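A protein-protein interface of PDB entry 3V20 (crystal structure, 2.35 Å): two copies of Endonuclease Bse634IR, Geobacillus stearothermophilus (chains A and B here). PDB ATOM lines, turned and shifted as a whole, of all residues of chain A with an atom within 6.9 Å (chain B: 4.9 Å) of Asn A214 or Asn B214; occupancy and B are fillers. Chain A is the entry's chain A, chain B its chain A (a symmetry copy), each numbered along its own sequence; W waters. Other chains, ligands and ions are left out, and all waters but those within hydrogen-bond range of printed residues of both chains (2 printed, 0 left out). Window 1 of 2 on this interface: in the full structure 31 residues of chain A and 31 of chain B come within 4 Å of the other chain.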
ATOM      1  N   LEU A 140      12.445  -0.220  20.403  1.00  0.00           N
ATOM      2  CA  LEU A 140      13.484  -0.421  21.420  1.00  0.00           C
ATOM      3  C   LEU A 140      14.007  -1.866  21.411  1.00  0.00           C
ATOM      4  O   LEU A 140      13.494  -2.708  22.137  1.00  0.00           O
ATOM      5  CB  LEU A 140      12.947  -0.069  22.812  1.00  0.00           C
ATOM      6  CG  LEU A 140      12.806   1.406  23.198  1.00  0.00           C
ATOM      7  CD1 LEU A 140      11.992   1.530  24.466  1.00  0.00           C
ATOM      8  CD2 LEU A 140      14.182   2.070  23.369  1.00  0.00           C
ATOM      9  N   LEU A 209      27.769  -4.061  25.264  1.00  0.00           N
ATOM     10  CA  LEU A 209      27.339  -4.120  26.665  1.00  0.00           C
ATOM     11  C   LEU A 209      26.660  -2.809  27.054  1.00  0.00           C
ATOM     12  O   LEU A 209      25.601  -2.824  27.685  1.00  0.00           O
ATOM     13  CB  LEU A 209      28.526  -4.409  27.595  1.00  0.00           C
ATOM     14  CG  LEU A 209      29.212  -5.781  27.426  1.00  0.00           C
ATOM     15  CD1 LEU A 209      30.681  -5.822  27.949  1.00  0.00           C
ATOM     16  CD2 LEU A 209      28.390  -6.880  28.060  1.00  0.00           C
ATOM     17  N   VAL A 210      27.258  -1.683  26.645  1.00  0.00           N
ATOM     18  CA  VAL A 210      26.698  -0.354  26.879  1.00  0.00           C
ATOM     19  C   VAL A 210      25.331  -0.174  26.208  1.00  0.00           C
ATOM     20  O   VAL A 210      24.386   0.296  26.835  1.00  0.00           O
ATOM     21  CB  VAL A 210      27.665   0.763  26.398  1.00  0.00           C
ATOM     22  CG1 VAL A 210      27.019   2.140  26.533  1.00  0.00           C
ATOM     23  CG2 VAL A 210      29.052   0.679  27.154  1.00  0.00           C
ATOM     24  N   HIS A 211      25.225  -0.536  24.936  1.00  0.00           N
ATOM     25  CA  HIS A 211      23.936  -0.463  24.262  1.00  0.00           C
ATOM     26  C   HIS A 211      22.860  -1.249  25.043  1.00  0.00           C
ATOM     27  O   HIS A 211      21.788  -0.725  25.366  1.00  0.00           O
ATOM     28  CB  HIS A 211      24.028  -0.968  22.831  1.00  0.00           C
ATOM     29  CG  HIS A 211      22.696  -1.094  22.165  1.00  0.00           C
ATOM     30  ND1 HIS A 211      21.970   0.004  21.749  1.00  0.00           N
ATOM     31  CD2 HIS A 211      21.932  -2.178  21.888  1.00  0.00           C
ATOM     32  CE1 HIS A 211      20.829  -0.403  21.221  1.00  0.00           C
ATOM     33  NE2 HIS A 211      20.781  -1.721  21.294  1.00  0.00           N
ATOM     34  N   GLU A 212      23.177  -2.497  25.353  1.00  0.00           N
ATOM     35  CA  GLU A 212      22.273  -3.384  26.094  1.00  0.00           C
ATOM     36  C   GLU A 212      21.741  -2.769  27.387  1.00  0.00           C
ATOM     37  O   GLU A 212      20.535  -2.749  27.604  1.00  0.00           O
ATOM     38  CB  GLU A 212      22.974  -4.698  26.393  1.00  0.00           C
ATOM     39  CG  GLU A 212      22.127  -5.695  27.118  1.00  0.00           C
ATOM     40  CD  GLU A 212      21.337  -6.570  26.184  1.00  0.00           C
ATOM     41  OE1 GLU A 212      21.706  -7.760  25.999  1.00  0.00           O
ATOM     42  OE2 GLU A 212      20.343  -6.061  25.630  1.00  0.00           O
ATOM     43  N   GLY A 213      22.653  -2.279  28.226  1.00  0.00           N
ATOM     44  CA  GLY A 213      22.313  -1.659  29.491  1.00  0.00           C
ATOM     45  C   GLY A 213      21.520  -0.378  29.307  1.00  0.00           C
ATOM     46  O   GLY A 213      20.606  -0.087  30.088  1.00  0.00           O
ATOM     47  N   ASN A 214      21.880   0.393  28.284  1.00  0.00           N
ATOM     48  CA  ASN A 214      21.135   1.578  27.942  1.00  0.00           C
ATOM     49  C   ASN A 214      19.687   1.249  27.604  1.00  0.00           C
ATOM     50  O   ASN A 214      18.774   1.906  28.105  1.00  0.00           O
ATOM     51  CB  ASN A 214      21.784   2.354  26.797  1.00  0.00           C
ATOM     52  CG  ASN A 214      21.247   3.757  26.689  1.00  0.00           C
ATOM     53  OD1 ASN A 214      21.209   4.492  27.679  1.00  0.00           O
ATOM     54  ND2 ASN A 214      20.822   4.143  25.498  1.00  0.00           N
ATOM     55  N   ILE A 215      19.472   0.235  26.776  1.00  0.00           N
ATOM     56  CA  ILE A 215      18.119  -0.118  26.371  1.00  0.00           C
ATOM     57  C   ILE A 215      17.299  -0.686  27.544  1.00  0.00           C
ATOM     58  O   ILE A 215      16.156  -0.277  27.757  1.00  0.00           O
ATOM     59  CB  ILE A 215      18.104  -1.075  25.142  1.00  0.00           C
ATOM     60  CG1 ILE A 215      18.881  -0.467  23.963  1.00  0.00           C
ATOM     61  CG2 ILE A 215      16.669  -1.408  24.706  1.00  0.00           C
ATOM     62  CD1 ILE A 215      18.425   0.918  23.542  1.00  0.00           C
ATOM     63  N   LEU A 216      17.883  -1.598  28.314  1.00  0.00           N
ATOM     64  CA  LEU A 216      17.185  -2.204  29.451  1.00  0.00           C
ATOM     65  C   LEU A 216      16.778  -1.182  30.514  1.00  0.00           C
ATOM     66  O   LEU A 216      15.716  -1.306  31.113  1.00  0.00           O
ATOM     67  CB  LEU A 216      18.049  -3.298  30.101  1.00  0.00           C
ATOM     68  CG  LEU A 216      18.454  -4.536  29.289  1.00  0.00           C
ATOM     69  CD1 LEU A 216      19.499  -5.360  30.043  1.00  0.00           C
ATOM     70  CD2 LEU A 216      17.244  -5.392  28.948  1.00  0.00           C
ATOM     71  N   LYS A 217      17.636  -0.193  30.756  1.00  0.00           N
ATOM     72  CA  LYS A 217      17.406   0.802  31.783  1.00  0.00           C
ATOM     73  C   LYS A 217      16.348   1.788  31.321  1.00  0.00           C
ATOM     74  O   LYS A 217      15.662   2.413  32.133  1.00  0.00           O
ATOM     75  CB  LYS A 217      18.707   1.536  32.140  1.00  0.00           C
ATOM     76  CG  LYS A 217      19.629   0.706  32.999  1.00  0.00           C
ATOM     77  CD  LYS A 217      20.896   1.421  33.431  1.00  0.00           C
ATOM     78  CE  LYS A 217      21.636   0.520  34.415  1.00  0.00           C
ATOM     79  NZ  LYS A 217      22.663   1.258  35.175  1.00  0.00           N
ATOM     80  N   SER A 218      16.240   1.920  30.007  1.00  0.00           N
ATOM     81  CA  SER A 218      15.267   2.801  29.385  1.00  0.00           C
ATOM     82  C   SER A 218      13.878   2.202  29.525  1.00  0.00           C
ATOM     83  O   SER A 218      12.946   2.899  29.935  1.00  0.00           O
ATOM     84  CB  SER A 218      15.611   3.013  27.915  1.00  0.00           C
ATOM     85  OG  SER A 218      14.837   4.063  27.393  1.00  0.00           O
ATOM     86  N   LEU A 219      13.749   0.911  29.208  1.00  0.00           N
ATOM     87  CA  LEU A 219      12.524   0.163  29.517  1.00  0.00           C
ATOM     88  C   LEU A 219      12.165   0.310  30.997  1.00  0.00           C
ATOM     89  O   LEU A 219      11.016   0.589  31.333  1.00  0.00           O
ATOM     90  CB  LEU A 219      12.656  -1.320  29.140  1.00  0.00           C
ATOM     91  CG  LEU A 219      12.767  -1.607  27.634  1.00  0.00           C
ATOM     92  CD1 LEU A 219      13.280  -3.033  27.360  1.00  0.00           C
ATOM     93  CD2 LEU A 219      11.436  -1.338  26.896  1.00  0.00           C
ATOM     94  N   TYR A 236      22.954  -3.123  35.555  1.00  0.00           N
ATOM     95  CA  TYR A 236      23.464  -3.966  34.483  1.00  0.00           C
ATOM     96  C   TYR A 236      24.973  -4.051  34.539  1.00  0.00           C
ATOM     97  O   TYR A 236      25.632  -3.045  34.800  1.00  0.00           O
ATOM     98  CB  TYR A 236      23.009  -3.436  33.130  1.00  0.00           C
ATOM     99  CG  TYR A 236      23.354  -4.349  31.985  1.00  0.00           C
ATOM    100  CD1 TYR A 236      22.632  -5.528  31.772  1.00  0.00           C
ATOM    101  CD2 TYR A 236      24.412  -4.052  31.119  1.00  0.00           C
ATOM    102  CE1 TYR A 236      22.942  -6.376  30.722  1.00  0.00           C
ATOM    103  CE2 TYR A 236      24.730  -4.906  30.056  1.00  0.00           C
ATOM    104  CZ  TYR A 236      23.985  -6.059  29.869  1.00  0.00           C
ATOM    105  OH  TYR A 236      24.267  -6.914  28.831  1.00  0.00           O
ATOM    106  N   THR A 254      30.378   4.574  30.219  1.00  0.00           N
ATOM    107  CA  THR A 254      29.507   5.406  29.393  1.00  0.00           C
ATOM    108  C   THR A 254      28.086   5.536  29.948  1.00  0.00           C
ATOM    109  O   THR A 254      27.461   4.546  30.352  1.00  0.00           O
ATOM    110  CB  THR A 254      29.527   4.922  27.945  1.00  0.00           C
ATOM    111  OG1 THR A 254      30.856   5.096  27.444  1.00  0.00           O
ATOM    112  CG2 THR A 254      28.574   5.716  27.058  1.00  0.00           C
ATOM    113  N   ALA A 255      27.584   6.769  29.944  1.00  0.00           N
ATOM    114  CA  ALA A 255      26.284   7.085  30.520  1.00  0.00           C
ATOM    115  C   ALA A 255      25.141   6.360  29.831  1.00  0.00           C
ATOM    116  O   ALA A 255      25.198   6.088  28.622  1.00  0.00           O
ATOM    117  CB  ALA A 255      26.036   8.592  30.456  1.00  0.00           C
ATOM    118  N   ALA A 256      24.111   6.050  30.609  1.00  0.00           N
ATOM    119  CA  ALA A 256      22.787   5.817  30.063  1.00  0.00           C
ATOM    120  C   ALA A 256      22.245   7.209  29.662  1.00  0.00           C
ATOM    121  O   ALA A 256      21.858   8.021  30.506  1.00  0.00           O
ATOM    122  CB  ALA A 256      21.889   5.152  31.109  1.00  0.00           C
ATOM    123  N   THR A 257      22.234   7.480  28.367  1.00  0.00           N
ATOM    124  CA  THR A 257      22.057   8.851  27.877  1.00  0.00           C
ATOM    125  C   THR A 257      20.806   9.627  28.343  1.00  0.00           C
ATOM    126  O   THR A 257      20.827  10.860  28.391  1.00  0.00           O
ATOM    127  CB  THR A 257      22.205   8.923  26.350  1.00  0.00           C
ATOM    128  OG1 THR A 257      21.365   7.932  25.753  1.00  0.00           O
ATOM    129  CG2 THR A 257      23.656   8.670  25.945  1.00  0.00           C
ATOM    130  N   HIS A 258      19.737   8.916  28.691  1.00  0.00           N
ATOM    131  CA  HIS A 258      18.512   9.563  29.164  1.00  0.00           C
ATOM    132  C   HIS A 258      18.669  10.129  30.585  1.00  0.00           C
ATOM    133  O   HIS A 258      17.800  10.860  31.077  1.00  0.00           O
ATOM    134  CB  HIS A 258      17.318   8.605  29.091  1.00  0.00           C
ATOM    135  CG  HIS A 258      17.401   7.454  30.042  1.00  0.00           C
ATOM    136  ND1 HIS A 258      17.977   6.248  29.701  1.00  0.00           N
ATOM    137  CD2 HIS A 258      16.986   7.324  31.324  1.00  0.00           C
ATOM    138  CE1 HIS A 258      17.915   5.426  30.737  1.00  0.00           C
ATOM    139  NE2 HIS A 258      17.320   6.056  31.735  1.00  0.00           N
ATOM    140  N   THR A 259      19.777   9.794  31.236  1.00  0.00           N
ATOM    141  CA  THR A 259      20.025  10.271  32.587  1.00  0.00           C
ATOM    142  C   THR A 259      20.916  11.516  32.623  1.00  0.00           C
ATOM    143  O   THR A 259      21.239  11.996  33.707  1.00  0.00           O
ATOM    144  CB  THR A 259      20.639   9.166  33.505  1.00  0.00           C
ATOM    145  OG1 THR A 259      21.952   8.832  33.048  1.00  0.00           O
ATOM    146  CG2 THR A 259      19.766   7.923  33.539  1.00  0.00           C
ATOM    147  N   GLU A 268      23.733   8.331  35.267  1.00  0.00           N
ATOM    148  CA  GLU A 268      23.816   6.899  35.525  1.00  0.00           C
ATOM    149  C   GLU A 268      24.611   6.199  34.414  1.00  0.00           C
ATOM    150  O   GLU A 268      24.423   6.495  33.234  1.00  0.00           O
ATOM    151  CB  GLU A 268      22.409   6.330  35.633  1.00  0.00           C
ATOM    152  CG  GLU A 268      22.333   4.882  36.054  1.00  0.00           C
ATOM    153  CD  GLU A 268      20.904   4.364  36.079  1.00  0.00           C
ATOM    154  OE1 GLU A 268      19.971   5.201  35.929  1.00  0.00           O
ATOM    155  OE2 GLU A 268      20.729   3.124  36.254  1.00  0.00           O
ATOM    156  N   ARG A 269      25.515   5.300  34.806  1.00  0.00           N
ATOM    157  CA  ARG A 269      26.274   4.459  33.868  1.00  0.00           C
ATOM    158  C   ARG A 269      25.315   3.446  33.245  1.00  0.00           C
ATOM    159  O   ARG A 269      24.404   2.958  33.923  1.00  0.00           O
ATOM    160  CB  ARG A 269      27.404   3.710  34.589  1.00  0.00           C
ATOM    161  CG  ARG A 269      28.631   4.564  34.950  1.00  0.00           C
ATOM    162  CD  ARG A 269      29.757   3.763  35.620  1.00  0.00           C
ATOM    163  NE  ARG A 269      30.060   2.513  34.908  1.00  0.00           N
ATOM    164  CZ  ARG A 269      30.994   1.627  35.273  1.00  0.00           C
ATOM    165  NH1 ARG A 269      31.762   1.836  36.347  1.00  0.00           N
ATOM    166  NH2 ARG A 269      31.171   0.528  34.548  1.00  0.00           N
ATOM    167  N   ALA A 270      25.507   3.139  31.966  1.00  0.00           N
ATOM    168  CA  ALA A 270      24.719   2.078  31.322  1.00  0.00           C
ATOM    169  C   ALA A 270      25.112   0.693  31.880  1.00  0.00           C
ATOM    170  O   ALA A 270      24.251  -0.162  32.110  1.00  0.00           O
ATOM    171  CB  ALA A 270      24.876   2.114  29.807  1.00  0.00           C
ATOM    172  N   VAL A 271      26.410   0.500  32.103  1.00  0.00           N
ATOM    173  CA  VAL A 271      26.929  -0.727  32.694  1.00  0.00           C
ATOM    174  C   VAL A 271      27.503  -0.327  34.038  1.00  0.00           C
ATOM    175  O   VAL A 271      28.480   0.421  34.108  1.00  0.00           O
ATOM    176  CB  VAL A 271      28.001  -1.415  31.780  1.00  0.00           C
ATOM    177  CG1 VAL A 271      28.443  -2.745  32.341  1.00  0.00           C
ATOM    178  CG2 VAL A 271      27.458  -1.610  30.364  1.00  0.00           C
ATOM    179  N   VAL B 210      23.645   1.650  16.276  1.00  0.00           N
ATOM    180  CA  VAL B 210      22.696   2.273  17.196  1.00  0.00           C
ATOM    181  C   VAL B 210      23.395   2.956  18.377  1.00  0.00           C
ATOM    182  O   VAL B 210      23.092   4.100  18.704  1.00  0.00           O
ATOM    183  CB  VAL B 210      21.661   1.243  17.728  1.00  0.00           C
ATOM    184  CG1 VAL B 210      20.754   1.876  18.781  1.00  0.00           C
ATOM    185  CG2 VAL B 210      20.839   0.598  16.542  1.00  0.00           C
ATOM    186  N   HIS B 211      24.320   2.259  19.023  1.00  0.00           N
ATOM    187  CA  HIS B 211      25.076   2.875  20.104  1.00  0.00           C
ATOM    188  C   HIS B 211      25.749   4.183  19.632  1.00  0.00           C
ATOM    189  O   HIS B 211      25.594   5.245  20.246  1.00  0.00           O
ATOM    190  CB  HIS B 211      26.114   1.920  20.672  1.00  0.00           C
ATOM    191  CG  HIS B 211      27.041   2.571  21.649  1.00  0.00           C
ATOM    192  ND1 HIS B 211      26.643   2.925  22.922  1.00  0.00           N
ATOM    193  CD2 HIS B 211      28.326   2.980  21.526  1.00  0.00           C
ATOM    194  CE1 HIS B 211      27.655   3.499  23.549  1.00  0.00           C
ATOM    195  NE2 HIS B 211      28.686   3.546  22.725  1.00  0.00           N
ATOM    196  N   GLU B 212      26.473   4.085  18.526  1.00  0.00           N
ATOM    197  CA  GLU B 212      27.178   5.230  17.937  1.00  0.00           C
ATOM    198  C   GLU B 212      26.288   6.453  17.731  1.00  0.00           C
ATOM    199  O   GLU B 212      26.635   7.543  18.170  1.00  0.00           O
ATOM    200  CB  GLU B 212      27.811   4.818  16.619  1.00  0.00           C
ATOM    201  CG  GLU B 212      28.589   5.905  15.946  1.00  0.00           C
ATOM    202  CD  GLU B 212      30.027   5.941  16.385  1.00  0.00           C
ATOM    203  OE1 GLU B 212      30.917   5.503  15.608  1.00  0.00           O
ATOM    204  OE2 GLU B 212      30.267   6.408  17.516  1.00  0.00           O
ATOM    205  N   GLY B 213      25.153   6.251  17.062  1.00  0.00           N
ATOM    206  CA  GLY B 213      24.198   7.306  16.787  1.00  0.00           C
ATOM    207  C   GLY B 213      23.573   7.859  18.054  1.00  0.00           C
ATOM    208  O   GLY B 213      23.328   9.066  18.159  1.00  0.00           O
ATOM    209  N   ASN B 214      23.302   6.972  19.010  1.00  0.00           N
ATOM    210  CA  ASN B 214      22.808   7.390  20.298  1.00  0.00           C
ATOM    211  C   ASN B 214      23.787   8.325  20.995  1.00  0.00           C
ATOM    212  O   ASN B 214      23.382   9.373  21.500  1.00  0.00           O
ATOM    213  CB  ASN B 214      22.479   6.200  21.198  1.00  0.00           C
ATOM    214  CG  ASN B 214      21.622   6.599  22.371  1.00  0.00           C
ATOM    215  OD1 ASN B 214      20.589   7.249  22.200  1.00  0.00           O
ATOM    216  ND2 ASN B 214      22.039   6.224  23.569  1.00  0.00           N
ATOM    217  N   ILE B 215      25.064   7.966  21.011  1.00  0.00           N
ATOM    218  CA  ILE B 215      26.057   8.785  21.691  1.00  0.00           C
ATOM    219  C   ILE B 215      26.274  10.133  20.980  1.00  0.00           C
ATOM    220  O   ILE B 215      26.289  11.181  21.627  1.00  0.00           O
ATOM    221  CB  ILE B 215      27.399   8.025  21.906  1.00  0.00           C
ATOM    222  CG1 ILE B 215      27.170   6.709  22.667  1.00  0.00           C
ATOM    223  CG2 ILE B 215      28.422   8.891  22.657  1.00  0.00           C
ATOM    224  CD1 ILE B 215      26.443   6.853  23.991  1.00  0.00           C
ATOM    225  N   LEU B 216      26.411  10.112  19.658  1.00  0.00           N
ATOM    226  CA  LEU B 216      26.628  11.340  18.888  1.00  0.00           C
ATOM    227  C   LEU B 216      25.475  12.336  19.018  1.00  0.00           C
ATOM    228  O   LEU B 216      25.701  13.540  19.057  1.00  0.00           O
ATOM    229  CB  LEU B 216      26.858  11.019  17.403  1.00  0.00           C
ATOM    230  CG  LEU B 216      28.067  10.170  16.981  1.00  0.00           C
ATOM    231  CD1 LEU B 216      27.964   9.776  15.507  1.00  0.00           C
ATOM    232  CD2 LEU B 216      29.373  10.901  17.249  1.00  0.00           C
ATOM    233  N   LYS B 217      24.244  11.828  19.060  1.00  0.00           N
ATOM    234  CA  LYS B 217      23.060  12.662  19.114  1.00  0.00           C
ATOM    235  C   LYS B 217      22.902  13.248  20.505  1.00  0.00           C
ATOM    236  O   LYS B 217      22.289  14.303  20.685  1.00  0.00           O
ATOM    237  CB  LYS B 217      21.807  11.865  18.719  1.00  0.00           C
ATOM    238  CG  LYS B 217      21.708  11.631  17.233  1.00  0.00           C
ATOM    239  CD  LYS B 217      20.448  10.906  16.794  1.00  0.00           C
ATOM    240  CE  LYS B 217      20.417  10.891  15.269  1.00  0.00           C
ATOM    241  NZ  LYS B 217      19.078  10.557  14.747  1.00  0.00           N
ATOM    242  N   SER B 218      23.455  12.540  21.479  1.00  0.00           N
ATOM    243  CA  SER B 218      23.424  12.959  22.869  1.00  0.00           C
ATOM    244  C   SER B 218      24.369  14.131  23.068  1.00  0.00           C
ATOM    245  O   SER B 218      23.983  15.139  23.665  1.00  0.00           O
ATOM    246  CB  SER B 218      23.812  11.799  23.779  1.00  0.00           C
ATOM    247  OG  SER B 218      23.522  12.125  25.115  1.00  0.00           O
ATOM    248  N   ALA B 255      15.258   3.622  19.137  1.00  0.00           N
ATOM    249  CA  ALA B 255      15.238   5.013  19.570  1.00  0.00           C
ATOM    250  C   ALA B 255      16.578   5.483  20.108  1.00  0.00           C
ATOM    251  O   ALA B 255      17.340   4.697  20.692  1.00  0.00           O
ATOM    252  CB  ALA B 255      14.167   5.212  20.642  1.00  0.00           C
ATOM    253  N   ALA B 256      16.856   6.765  19.904  1.00  0.00           N
ATOM    254  CA  ALA B 256      17.808   7.479  20.735  1.00  0.00           C
ATOM    255  C   ALA B 256      17.101   7.704  22.092  1.00  0.00           C
ATOM    256  O   ALA B 256      16.208   8.546  22.224  1.00  0.00           O
ATOM    257  CB  ALA B 256      18.192   8.809  20.082  1.00  0.00           C
ATOM    258  N   THR B 257      17.497   6.934  23.092  1.00  0.00           N
ATOM    259  CA  THR B 257      16.707   6.815  24.321  1.00  0.00           C
ATOM    260  C   THR B 257      16.354   8.112  25.081  1.00  0.00           C
ATOM    261  O   THR B 257      15.344   8.158  25.788  1.00  0.00           O
ATOM    262  CB  THR B 257      17.309   5.772  25.275  1.00  0.00           C
ATOM    263  OG1 THR B 257      18.701   6.050  25.450  1.00  0.00           O
ATOM    264  CG2 THR B 257      17.140   4.367  24.700  1.00  0.00           C
ATOM    265  N   HIS B 258      17.168   9.153  24.927  1.00  0.00           N
ATOM    266  CA  HIS B 258      16.904  10.431  25.592  1.00  0.00           C
ATOM    267  C   HIS B 258      15.728  11.184  24.950  1.00  0.00           C
ATOM    268  O   HIS B 258      15.251  12.193  25.486  1.00  0.00           O
ATOM    269  CB  HIS B 258      18.160  11.309  25.618  1.00  0.00           C
ATOM    270  CG  HIS B 258      18.596  11.789  24.270  1.00  0.00           C
ATOM    271  ND1 HIS B 258      19.492  11.092  23.486  1.00  0.00           N
ATOM    272  CD2 HIS B 258      18.258  12.893  23.564  1.00  0.00           C
ATOM    273  CE1 HIS B 258      19.683  11.748  22.352  1.00  0.00           C
ATOM    274  NE2 HIS B 258      18.943  12.843  22.374  1.00  0.00           N
ATOM    275  N   ALA B 270      17.994   6.401  16.612  1.00  0.00           N
ATOM    276  CA  ALA B 270      19.442   6.607  16.752  1.00  0.00           C
ATOM    277  C   ALA B 270      20.129   6.597  15.368  1.00  0.00           C
ATOM    278  O   ALA B 270      21.032   7.397  15.106  1.00  0.00           O
ATOM    279  CB  ALA B 270      20.064   5.564  17.671  1.00  0.00           C
HETATM  280  O   HOH W   1      14.817   6.632  27.978  1.00  0.00           O
HETATM  281  O   HOH W   2      21.214  12.566  26.307  1.00  0.00           O
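The side-chain amide nitrogen (ND2) of Asn A214 lies within hydrogen-bond range of the side-chain hydroxyl (OG1) of Thr B257, at 2.9 Å. ND2 of Asn B214 sits close to ND2 of Asn A214 (3.1 Å). The side-chain hydroxyl (OG1) of Thr B257 lies within hydrogen-bond range of the side-chain hydroxyl (OG1) of Thr A257 (3.3 Å). The side-chain hydroxyl (OG1) of Thr A257 sits at hydrogen-bond distance from the side-chain amide nitrogen (ND2) of Asn B214, 2.9 Å away.
The side-chain amide oxygen of Asn B214 lies within hydrogen-bond range of the backbone NH of Thr B257 (3.2 Å). The backbone NH of Ala A270 sits at hydrogen-bond distance from the backbone carbonyl oxygen of Thr A254 (2.9 Å). The backbone NH (N) of Thr A257 lies within hydrogen-bond range of the side-chain amide oxygen (OD1) of Asn A214 (3.2 Å).
CG2 of Thr B257 touches CD2 of Leu A140, at 3.97 Å. CG1 of Val A210 touches CE1 of His B211, 3.3 Å away. Val B210 touches His A211. Thr B257 touches Ile A215 (CG2 to CD1, 3.9 Å). Ser A218 touches Thr B257 (OG to CG2, 3.6 Å). Ile B215 touches Thr A254. Ile B215 touches Thr A257. Thr A257 touches Ser B218 (CG2 to OG, 3.6 Å). O of Thr B257 touches CB of His A258, at 3.9 Å. CA of His A258 touches CB of His B258, 3.97 Å away.
Asn A214 touches just these residues of chain B: Asn B214 and Thr B257. Printed residues of chain B within 4 Å of Thr A254: Ile B215. Printed residues of chain B within 4 Å of His A258: Thr B257 and His B258. No residue of chain A comes within 4 Å of Gly B213. Of chain A, only Asn A214 (3.1 Å) and Thr A257 (2.9 Å) come within 4 Å of Asn B214. The nearest residue of chain A that does not touch Asn B214 is Ala A255 (6.0 Å).
Hydrophobic or aromatic side chains of chain A within 4 Å of the printed part of chain B: Leu A140, Val A210, His A211, Ile A215 and His A258. Along chain A the printed residues that touch a printed residue of chain B span positions 140 to 258. Of the 14 printed residues of chain B, 7 touch a printed residue of chain A. Printed residues of chain B that touch a printed residue of chain A: Val B210, His B211, Asn B214, Ile B215, Ser B218, Thr B257 and His B258. Hydrophobic or aromatic side chains of chain B that line the printed part of chain A: Val B210, His B211, Ile B215 and His B258. Along chain B the printed residues that touch a printed residue of chain A span positions 210 to 258. Among the printed residues, 15 pairs touch across the chains. Among the printed residues, no Asp or Glu carboxylate lies within 4 Å of a Lys or Arg side-chain nitrogen of the other chain.
Val A210 touches His B211, and with the chains exchanged His A211 touches Val B210. Asn B214 touches its own counterpart, Asn A214. Ser A218 touches Thr B257, and with the chains exchanged Thr A257 touches Ser B218. His A258 touches its own counterpart, His B258. Positions printed for both chains: 210, 211, 212, 213, 214, 215, 216, 217, 218, 255, 256, 257, 258 and 270. Of the 15 pairs that touch across the chains among the printed residues, 13 have their exchanged pair printed and touching as well.
Water W2 bridges the side-chain hydroxyl of Ser B218 (2.6 Å) and the backbone carbonyl oxygen of Thr A257 (2.7 Å). Water W1 bridges OG of Ser A218 and O of Thr B257.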
